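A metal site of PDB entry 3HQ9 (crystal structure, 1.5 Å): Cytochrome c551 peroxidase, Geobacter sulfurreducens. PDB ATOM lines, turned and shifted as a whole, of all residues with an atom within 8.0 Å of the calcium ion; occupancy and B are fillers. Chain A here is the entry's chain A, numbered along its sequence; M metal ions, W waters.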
ATOM      1  N   GLY A  84     -24.098 -13.822  26.074  1.00  0.00           N
ATOM      2  CA  GLY A  84     -24.785 -13.006  25.082  1.00  0.00           C
ATOM      3  C   GLY A  84     -26.080 -12.434  25.636  1.00  0.00           C
ATOM      4  O   GLY A  84     -26.247 -12.290  26.849  1.00  0.00           O
ATOM      5  N   ASP A  85     -27.007 -12.090  24.740  1.00  0.00           N
ATOM      6  CA  ASP A  85     -28.227 -11.353  25.139  1.00  0.00           C
ATOM      7  C   ASP A  85     -29.567 -11.919  24.635  1.00  0.00           C
ATOM      8  O   ASP A  85     -30.602 -11.315  24.912  1.00  0.00           O
ATOM      9  CB  ASP A  85     -28.127  -9.875  24.742  1.00  0.00           C
ATOM     10  CG  ASP A  85     -28.136  -9.648  23.243  1.00  0.00           C
ATOM     11  OD1 ASP A  85     -28.200 -10.634  22.457  1.00  0.00           O
ATOM     12  OD2 ASP A  85     -28.100  -8.472  22.807  1.00  0.00           O
ATOM     13  N   LEU A  86     -29.517 -13.052  23.953  1.00  0.00           N
ATOM     14  CA  LEU A  86     -30.716 -13.757  23.459  1.00  0.00           C
ATOM     15  C   LEU A  86     -31.416 -13.030  22.325  1.00  0.00           C
ATOM     16  O   LEU A  86     -32.541 -13.375  22.017  1.00  0.00           O
ATOM     17  CB  LEU A  86     -31.749 -13.960  24.586  1.00  0.00           C
ATOM     18  CG  LEU A  86     -31.315 -14.576  25.918  1.00  0.00           C
ATOM     19  CD1 LEU A  86     -32.489 -14.683  26.931  1.00  0.00           C
ATOM     20  CD2 LEU A  86     -30.690 -15.924  25.644  1.00  0.00           C
ATOM     21  N   GLN A  87     -30.758 -12.030  21.729  1.00  0.00           N
ATOM     22  CA  GLN A  87     -31.386 -11.161  20.729  1.00  0.00           C
ATOM     23  C   GLN A  87     -30.801 -11.342  19.344  1.00  0.00           C
ATOM     24  O   GLN A  87     -29.655 -11.743  19.176  1.00  0.00           O
ATOM     25  CB  GLN A  87     -31.201  -9.675  21.110  1.00  0.00           C
ATOM     26  CG  GLN A  87     -31.672  -9.338  22.508  1.00  0.00           C
ATOM     27  CD  GLN A  87     -33.171  -9.386  22.664  1.00  0.00           C
ATOM     28  OE1 GLN A  87     -33.905  -8.904  21.794  1.00  0.00           O
ATOM     29  NE2 GLN A  87     -33.653  -9.936  23.783  1.00  0.00           N
ATOM     30  N   ALA A  88     -31.609 -11.022  18.328  1.00  0.00           N
ATOM     31  CA  ALA A  88     -31.104 -10.984  16.960  1.00  0.00           C
ATOM     32  C   ALA A  88     -29.998  -9.931  16.867  1.00  0.00           C
ATOM     33  O   ALA A  88     -28.868 -10.233  16.467  1.00  0.00           O
ATOM     34  CB  ALA A  88     -32.244 -10.680  15.979  1.00  0.00           C
ATOM     35  N   ASN A 101     -25.469  -8.503  16.211  1.00  0.00           N
ATOM     36  CA  ASN A 101     -25.676  -9.492  17.236  1.00  0.00           C
ATOM     37  C   ASN A 101     -24.554  -9.362  18.266  1.00  0.00           C
ATOM     38  O   ASN A 101     -23.402  -9.135  17.898  1.00  0.00           O
ATOM     39  CB  ASN A 101     -25.644 -10.861  16.546  1.00  0.00           C
ATOM     40  CG  ASN A 101     -25.942 -12.007  17.474  1.00  0.00           C
ATOM     41  OD1 ASN A 101     -25.026 -12.725  17.891  1.00  0.00           O
ATOM     42  ND2 ASN A 101     -27.197 -12.141  17.853  1.00  0.00           N
ATOM     43  N   ALA A 102     -24.882  -9.462  19.540  1.00  0.00           N
ATOM     44  CA  ALA A 102     -23.852  -9.414  20.564  1.00  0.00           C
ATOM     45  C   ALA A 102     -23.094 -10.736  20.614  1.00  0.00           C
ATOM     46  O   ALA A 102     -23.701 -11.793  20.881  1.00  0.00           O
ATOM     47  CB  ALA A 102     -24.452  -9.076  21.941  1.00  0.00           C
ATOM     48  N   PRO A 103     -21.784 -10.701  20.348  1.00  0.00           N
ATOM     49  CA  PRO A 103     -20.962 -11.901  20.476  1.00  0.00           C
ATOM     50  C   PRO A 103     -20.741 -12.225  21.927  1.00  0.00           C
ATOM     51  O   PRO A 103     -20.840 -11.338  22.791  1.00  0.00           O
ATOM     52  CB  PRO A 103     -19.651 -11.509  19.807  1.00  0.00           C
ATOM     53  CG  PRO A 103     -19.554 -10.045  20.106  1.00  0.00           C
ATOM     54  CD  PRO A 103     -20.944  -9.508  20.115  1.00  0.00           C
ATOM     55  N   THR A 104     -20.503 -13.491  22.219  1.00  0.00           N
ATOM     56  CA  THR A 104     -20.324 -13.899  23.593  1.00  0.00           C
ATOM     57  C   THR A 104     -19.032 -13.343  24.198  1.00  0.00           C
ATOM     58  O   THR A 104     -17.996 -13.259  23.540  1.00  0.00           O
ATOM     59  CB  THR A 104     -20.350 -15.442  23.748  1.00  0.00           C
ATOM     60  OG1 THR A 104     -20.258 -15.760  25.137  1.00  0.00           O
ATOM     61  CG2 THR A 104     -19.193 -16.130  23.015  1.00  0.00           C
ATOM     62  N   TRP A 116     -17.254  -7.646  14.124  1.00  0.00           N
ATOM     63  CA  TRP A 116     -18.019  -8.564  13.268  1.00  0.00           C
ATOM     64  C   TRP A 116     -17.629  -8.396  11.803  1.00  0.00           C
ATOM     65  O   TRP A 116     -17.591  -9.373  11.060  1.00  0.00           O
ATOM     66  CB  TRP A 116     -19.507  -8.311  13.383  1.00  0.00           C
ATOM     67  CG  TRP A 116     -20.226  -9.168  14.329  1.00  0.00           C
ATOM     68  CD1 TRP A 116     -20.868  -8.785  15.472  1.00  0.00           C
ATOM     69  CD2 TRP A 116     -20.481 -10.565  14.172  1.00  0.00           C
ATOM     70  NE1 TRP A 116     -21.481  -9.866  16.058  1.00  0.00           N
ATOM     71  CE2 TRP A 116     -21.262 -10.964  15.283  1.00  0.00           C
ATOM     72  CE3 TRP A 116     -20.111 -11.520  13.223  1.00  0.00           C
ATOM     73  CZ2 TRP A 116     -21.689 -12.278  15.448  1.00  0.00           C
ATOM     74  CZ3 TRP A 116     -20.543 -12.827  13.392  1.00  0.00           C
ATOM     75  CH2 TRP A 116     -21.322 -13.196  14.497  1.00  0.00           C
ATOM     76  N   PRO A 270     -16.417 -16.304  13.386  1.00  0.00           N
ATOM     77  CA  PRO A 270     -16.427 -16.326  14.846  1.00  0.00           C
ATOM     78  C   PRO A 270     -15.898 -17.629  15.462  1.00  0.00           C
ATOM     79  O   PRO A 270     -15.934 -18.693  14.845  1.00  0.00           O
ATOM     80  CB  PRO A 270     -17.908 -16.155  15.201  1.00  0.00           C
ATOM     81  CG  PRO A 270     -18.536 -15.632  14.003  1.00  0.00           C
ATOM     82  CD  PRO A 270     -17.788 -16.228  12.868  1.00  0.00           C
ATOM     83  N   ASN A 274     -19.080 -22.714  22.503  1.00  0.00           N
ATOM     84  CA  ASN A 274     -20.401 -22.429  23.073  1.00  0.00           C
ATOM     85  C   ASN A 274     -21.461 -22.015  22.075  1.00  0.00           C
ATOM     86  O   ASN A 274     -22.485 -21.449  22.460  1.00  0.00           O
ATOM     87  CB  ASN A 274     -20.285 -21.392  24.184  1.00  0.00           C
ATOM     88  CG  ASN A 274     -19.434 -21.875  25.326  1.00  0.00           C
ATOM     89  OD1 ASN A 274     -19.809 -22.844  26.014  1.00  0.00           O
ATOM     90  ND2 ASN A 274     -18.271 -21.254  25.514  1.00  0.00           N
ATOM     91  N   VAL A 275     -21.235 -22.294  20.794  1.00  0.00           N
ATOM     92  CA  VAL A 275     -22.152 -21.795  19.753  1.00  0.00           C
ATOM     93  C   VAL A 275     -23.585 -22.300  19.958  1.00  0.00           C
ATOM     94  O   VAL A 275     -24.543 -21.596  19.660  1.00  0.00           O
ATOM     95  CB  VAL A 275     -21.653 -22.127  18.326  1.00  0.00           C
ATOM     96  CG1 VAL A 275     -21.583 -23.643  18.110  1.00  0.00           C
ATOM     97  CG2 VAL A 275     -22.535 -21.475  17.272  1.00  0.00           C
ATOM     98  N   ILE A 277     -25.244 -22.381  22.548  1.00  0.00           N
ATOM     99  CA  ILE A 277     -25.950 -21.541  23.524  1.00  0.00           C
ATOM    100  C   ILE A 277     -25.825 -20.032  23.242  1.00  0.00           C
ATOM    101  O   ILE A 277     -26.227 -19.222  24.065  1.00  0.00           O
ATOM    102  CB  ILE A 277     -25.578 -21.858  25.011  1.00  0.00           C
ATOM    103  CG1 ILE A 277     -24.114 -21.585  25.319  1.00  0.00           C
ATOM    104  CG2 ILE A 277     -25.926 -23.310  25.326  1.00  0.00           C
ATOM    105  CD1 ILE A 277     -23.807 -21.594  26.782  1.00  0.00           C
ATOM    106  N   THR A 278     -25.335 -19.666  22.063  1.00  0.00           N
ATOM    107  CA  THR A 278     -25.182 -18.248  21.710  1.00  0.00           C
ATOM    108  C   THR A 278     -26.004 -17.868  20.464  1.00  0.00           C
ATOM    109  O   THR A 278     -25.718 -16.916  19.770  1.00  0.00           O
ATOM    110  CB  THR A 278     -23.706 -17.865  21.531  1.00  0.00           C
ATOM    111  OG1 THR A 278     -23.171 -18.588  20.433  1.00  0.00           O
ATOM    112  CG2 THR A 278     -22.884 -18.195  22.777  1.00  0.00           C
ATOM    113  N   TYR A 279     -27.061 -18.613  20.225  1.00  0.00           N
ATOM    114  CA  TYR A 279     -28.080 -18.269  19.243  1.00  0.00           C
ATOM    115  C   TYR A 279     -28.632 -16.864  19.525  1.00  0.00           C
ATOM    116  O   TYR A 279     -28.556 -16.368  20.661  1.00  0.00           O
ATOM    117  CB  TYR A 279     -29.235 -19.295  19.315  1.00  0.00           C
ATOM    118  CG  TYR A 279     -29.803 -19.375  20.717  1.00  0.00           C
ATOM    119  CD1 TYR A 279     -30.796 -18.498  21.131  1.00  0.00           C
ATOM    120  CD2 TYR A 279     -29.307 -20.288  21.647  1.00  0.00           C
ATOM    121  CE1 TYR A 279     -31.274 -18.499  22.389  1.00  0.00           C
ATOM    122  CE2 TYR A 279     -29.773 -20.296  22.942  1.00  0.00           C
ATOM    123  CZ  TYR A 279     -30.764 -19.404  23.294  1.00  0.00           C
ATOM    124  OH  TYR A 279     -31.251 -19.385  24.581  1.00  0.00           O
ATOM    125  N   PRO A 280     -29.214 -16.199  18.511  1.00  0.00           N
ATOM    126  CA  PRO A 280     -29.200 -16.584  17.098  1.00  0.00           C
ATOM    127  C   PRO A 280     -27.828 -16.293  16.495  1.00  0.00           C
ATOM    128  O   PRO A 280     -26.935 -15.782  17.195  1.00  0.00           O
ATOM    129  CB  PRO A 280     -30.288 -15.713  16.501  1.00  0.00           C
ATOM    130  CG  PRO A 280     -30.306 -14.502  17.380  1.00  0.00           C
ATOM    131  CD  PRO A 280     -29.998 -14.987  18.748  1.00  0.00           C
ATOM    132  N   TYR A 281     -27.685 -16.612  15.213  1.00  0.00           N
ATOM    133  CA  TYR A 281     -26.386 -16.736  14.553  1.00  0.00           C
ATOM    134  C   TYR A 281     -26.179 -15.736  13.444  1.00  0.00           C
ATOM    135  O   TYR A 281     -27.135 -15.169  12.903  1.00  0.00           O
ATOM    136  CB  TYR A 281     -26.238 -18.180  14.045  1.00  0.00           C
ATOM    137  CG  TYR A 281     -26.390 -19.144  15.185  1.00  0.00           C
ATOM    138  CD1 TYR A 281     -25.447 -19.201  16.207  1.00  0.00           C
ATOM    139  CD2 TYR A 281     -27.493 -20.000  15.262  1.00  0.00           C
ATOM    140  CE1 TYR A 281     -25.599 -20.031  17.266  1.00  0.00           C
ATOM    141  CE2 TYR A 281     -27.650 -20.853  16.340  1.00  0.00           C
ATOM    142  CZ  TYR A 281     -26.697 -20.880  17.332  1.00  0.00           C
ATOM    143  OH  TYR A 281     -26.841 -21.735  18.405  1.00  0.00           O
ATOM    144  N   PHE A 282     -24.890 -15.540  13.152  1.00  0.00           N
ATOM    145  CA  PHE A 282     -24.345 -14.602  12.196  1.00  0.00           C
ATOM    146  C   PHE A 282     -24.415 -13.175  12.716  1.00  0.00           C
ATOM    147  O   PHE A 282     -24.977 -12.923  13.784  1.00  0.00           O
ATOM    148  CB  PHE A 282     -24.962 -14.764  10.815  1.00  0.00           C
ATOM    149  CG  PHE A 282     -24.924 -16.188  10.328  1.00  0.00           C
ATOM    150  CD1 PHE A 282     -23.702 -16.836  10.203  1.00  0.00           C
ATOM    151  CD2 PHE A 282     -26.089 -16.873  10.019  1.00  0.00           C
ATOM    152  CE1 PHE A 282     -23.636 -18.144   9.783  1.00  0.00           C
ATOM    153  CE2 PHE A 282     -26.022 -18.207   9.572  1.00  0.00           C
ATOM    154  CZ  PHE A 282     -24.804 -18.827   9.465  1.00  0.00           C
ATOM    155  N   HIS A 283     -23.796 -12.285  11.961  1.00  0.00           N
ATOM    156  CA  HIS A 283     -23.551 -10.921  12.395  1.00  0.00           C
ATOM    157  C   HIS A 283     -24.848 -10.155  12.697  1.00  0.00           C
ATOM    158  O   HIS A 283     -24.867  -9.277  13.554  1.00  0.00           O
ATOM    159  CB  HIS A 283     -22.713 -10.170  11.345  1.00  0.00           C
ATOM    160  CG  HIS A 283     -23.461  -9.861  10.081  1.00  0.00           C
ATOM    161  ND1 HIS A 283     -23.572 -10.763   9.048  1.00  0.00           N
ATOM    162  CD2 HIS A 283     -24.168  -8.763   9.710  1.00  0.00           C
ATOM    163  CE1 HIS A 283     -24.316 -10.223   8.086  1.00  0.00           C
ATOM    164  NE2 HIS A 283     -24.690  -9.020   8.462  1.00  0.00           N
ATOM    165  N   SER A 284     -25.923 -10.524  11.979  1.00  0.00           N
ATOM    166  CA  SER A 284     -27.244  -9.923  12.064  1.00  0.00           C
ATOM    167  C   SER A 284     -28.247 -10.748  12.887  1.00  0.00           C
ATOM    168  O   SER A 284     -29.395 -10.352  13.033  1.00  0.00           O
ATOM    169  CB  SER A 284     -27.772  -9.822  10.641  1.00  0.00           C
ATOM    170  OG  SER A 284     -27.644 -11.096  10.023  1.00  0.00           O
ATOM    171  N   GLY A 285     -27.816 -11.878  13.452  1.00  0.00           N
ATOM    172  CA  GLY A 285     -28.691 -12.709  14.273  1.00  0.00           C
ATOM    173  C   GLY A 285     -29.936 -13.176  13.530  1.00  0.00           C
ATOM    174  O   GLY A 285     -31.016 -13.271  14.115  1.00  0.00           O
ATOM    175  N   VAL A 286     -29.780 -13.462  12.249  1.00  0.00           N
ATOM    176  CA  VAL A 286     -30.908 -13.764  11.380  1.00  0.00           C
ATOM    177  C   VAL A 286     -31.313 -15.238  11.388  1.00  0.00           C
ATOM    178  O   VAL A 286     -32.443 -15.568  10.976  1.00  0.00           O
ATOM    179  CB  VAL A 286     -30.620 -13.369   9.910  1.00  0.00           C
ATOM    180  CG1 VAL A 286     -30.687 -11.842   9.740  1.00  0.00           C
ATOM    181  CG2 VAL A 286     -29.275 -13.955   9.433  1.00  0.00           C
ATOM    182  N   VAL A 287     -30.412 -16.111  11.790  1.00  0.00           N
ATOM    183  CA  VAL A 287     -30.680 -17.538  11.836  1.00  0.00           C
ATOM    184  C   VAL A 287     -30.684 -18.055  13.282  1.00  0.00           C
ATOM    185  O   VAL A 287     -29.663 -17.979  13.982  1.00  0.00           O
ATOM    186  CB  VAL A 287     -29.656 -18.331  10.998  1.00  0.00           C
ATOM    187  CG1 VAL A 287     -29.861 -19.826  11.181  1.00  0.00           C
ATOM    188  CG2 VAL A 287     -29.784 -17.956   9.504  1.00  0.00           C
HETATM  189 CA    CA M   1     -25.058 -15.081  18.447  1.00  0.00          CA
HETATM  190  O   HOH W   1     -23.453 -16.847  18.176  1.00  0.00           O
HETATM  191  O   HOH W   2     -26.773 -14.206  19.955  1.00  0.00           O
HETATM  192  O   HOH W   3     -23.624 -14.302  20.155  1.00  0.00           O
HETATM  193  O   HOH W   4     -23.882 -14.776  16.324  1.00  0.00           O
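O of Thr 278 binds the calcium ion (2.4 Å).
O of Pro 280 binds the calcium ion (2.4 Å).
Water W3 is bound to the calcium ion (2.4 Å).
Water W1 binds the calcium ion (2.4 Å).
The calcium ion is bound by the side-chain amide oxygen (OD1) of Asn 101 (2.4 Å).
Water W4 binds the calcium ion (2.4 Å).
The calcium ion is bound by water W2 (2.4 Å).
The backbone carbonyl oxygen (O) of Asn 101 is in hydrogen-bond range of the indole nitrogen (NE1) of Trp 116 (2.8 Å).
N of Asn 101 is in hydrogen-bond range of O of His 283 (2.8 Å).
The side-chain hydroxyl (OG1) of Thr 278 sits at hydrogen-bond distance from the backbone carbonyl oxygen (O) of Val 275 (3.4 Å).
The backbone carbonyl oxygen of Gln 87 sits at hydrogen-bond distance from the side-chain amide nitrogen of Asn 101.
ND2 of Asn 101 lies within hydrogen-bond range of O of Ala 88 (2.9 Å).
Water W2 lies within hydrogen-bond range of the backbone carbonyl oxygen (O) of Tyr 279 (2.9 Å) and the side-chain amide nitrogen (ND2) of Asn 101 (3.0 Å).
Along chain A the residues within 4 Å of the calcium ion span positions 101 to 280.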
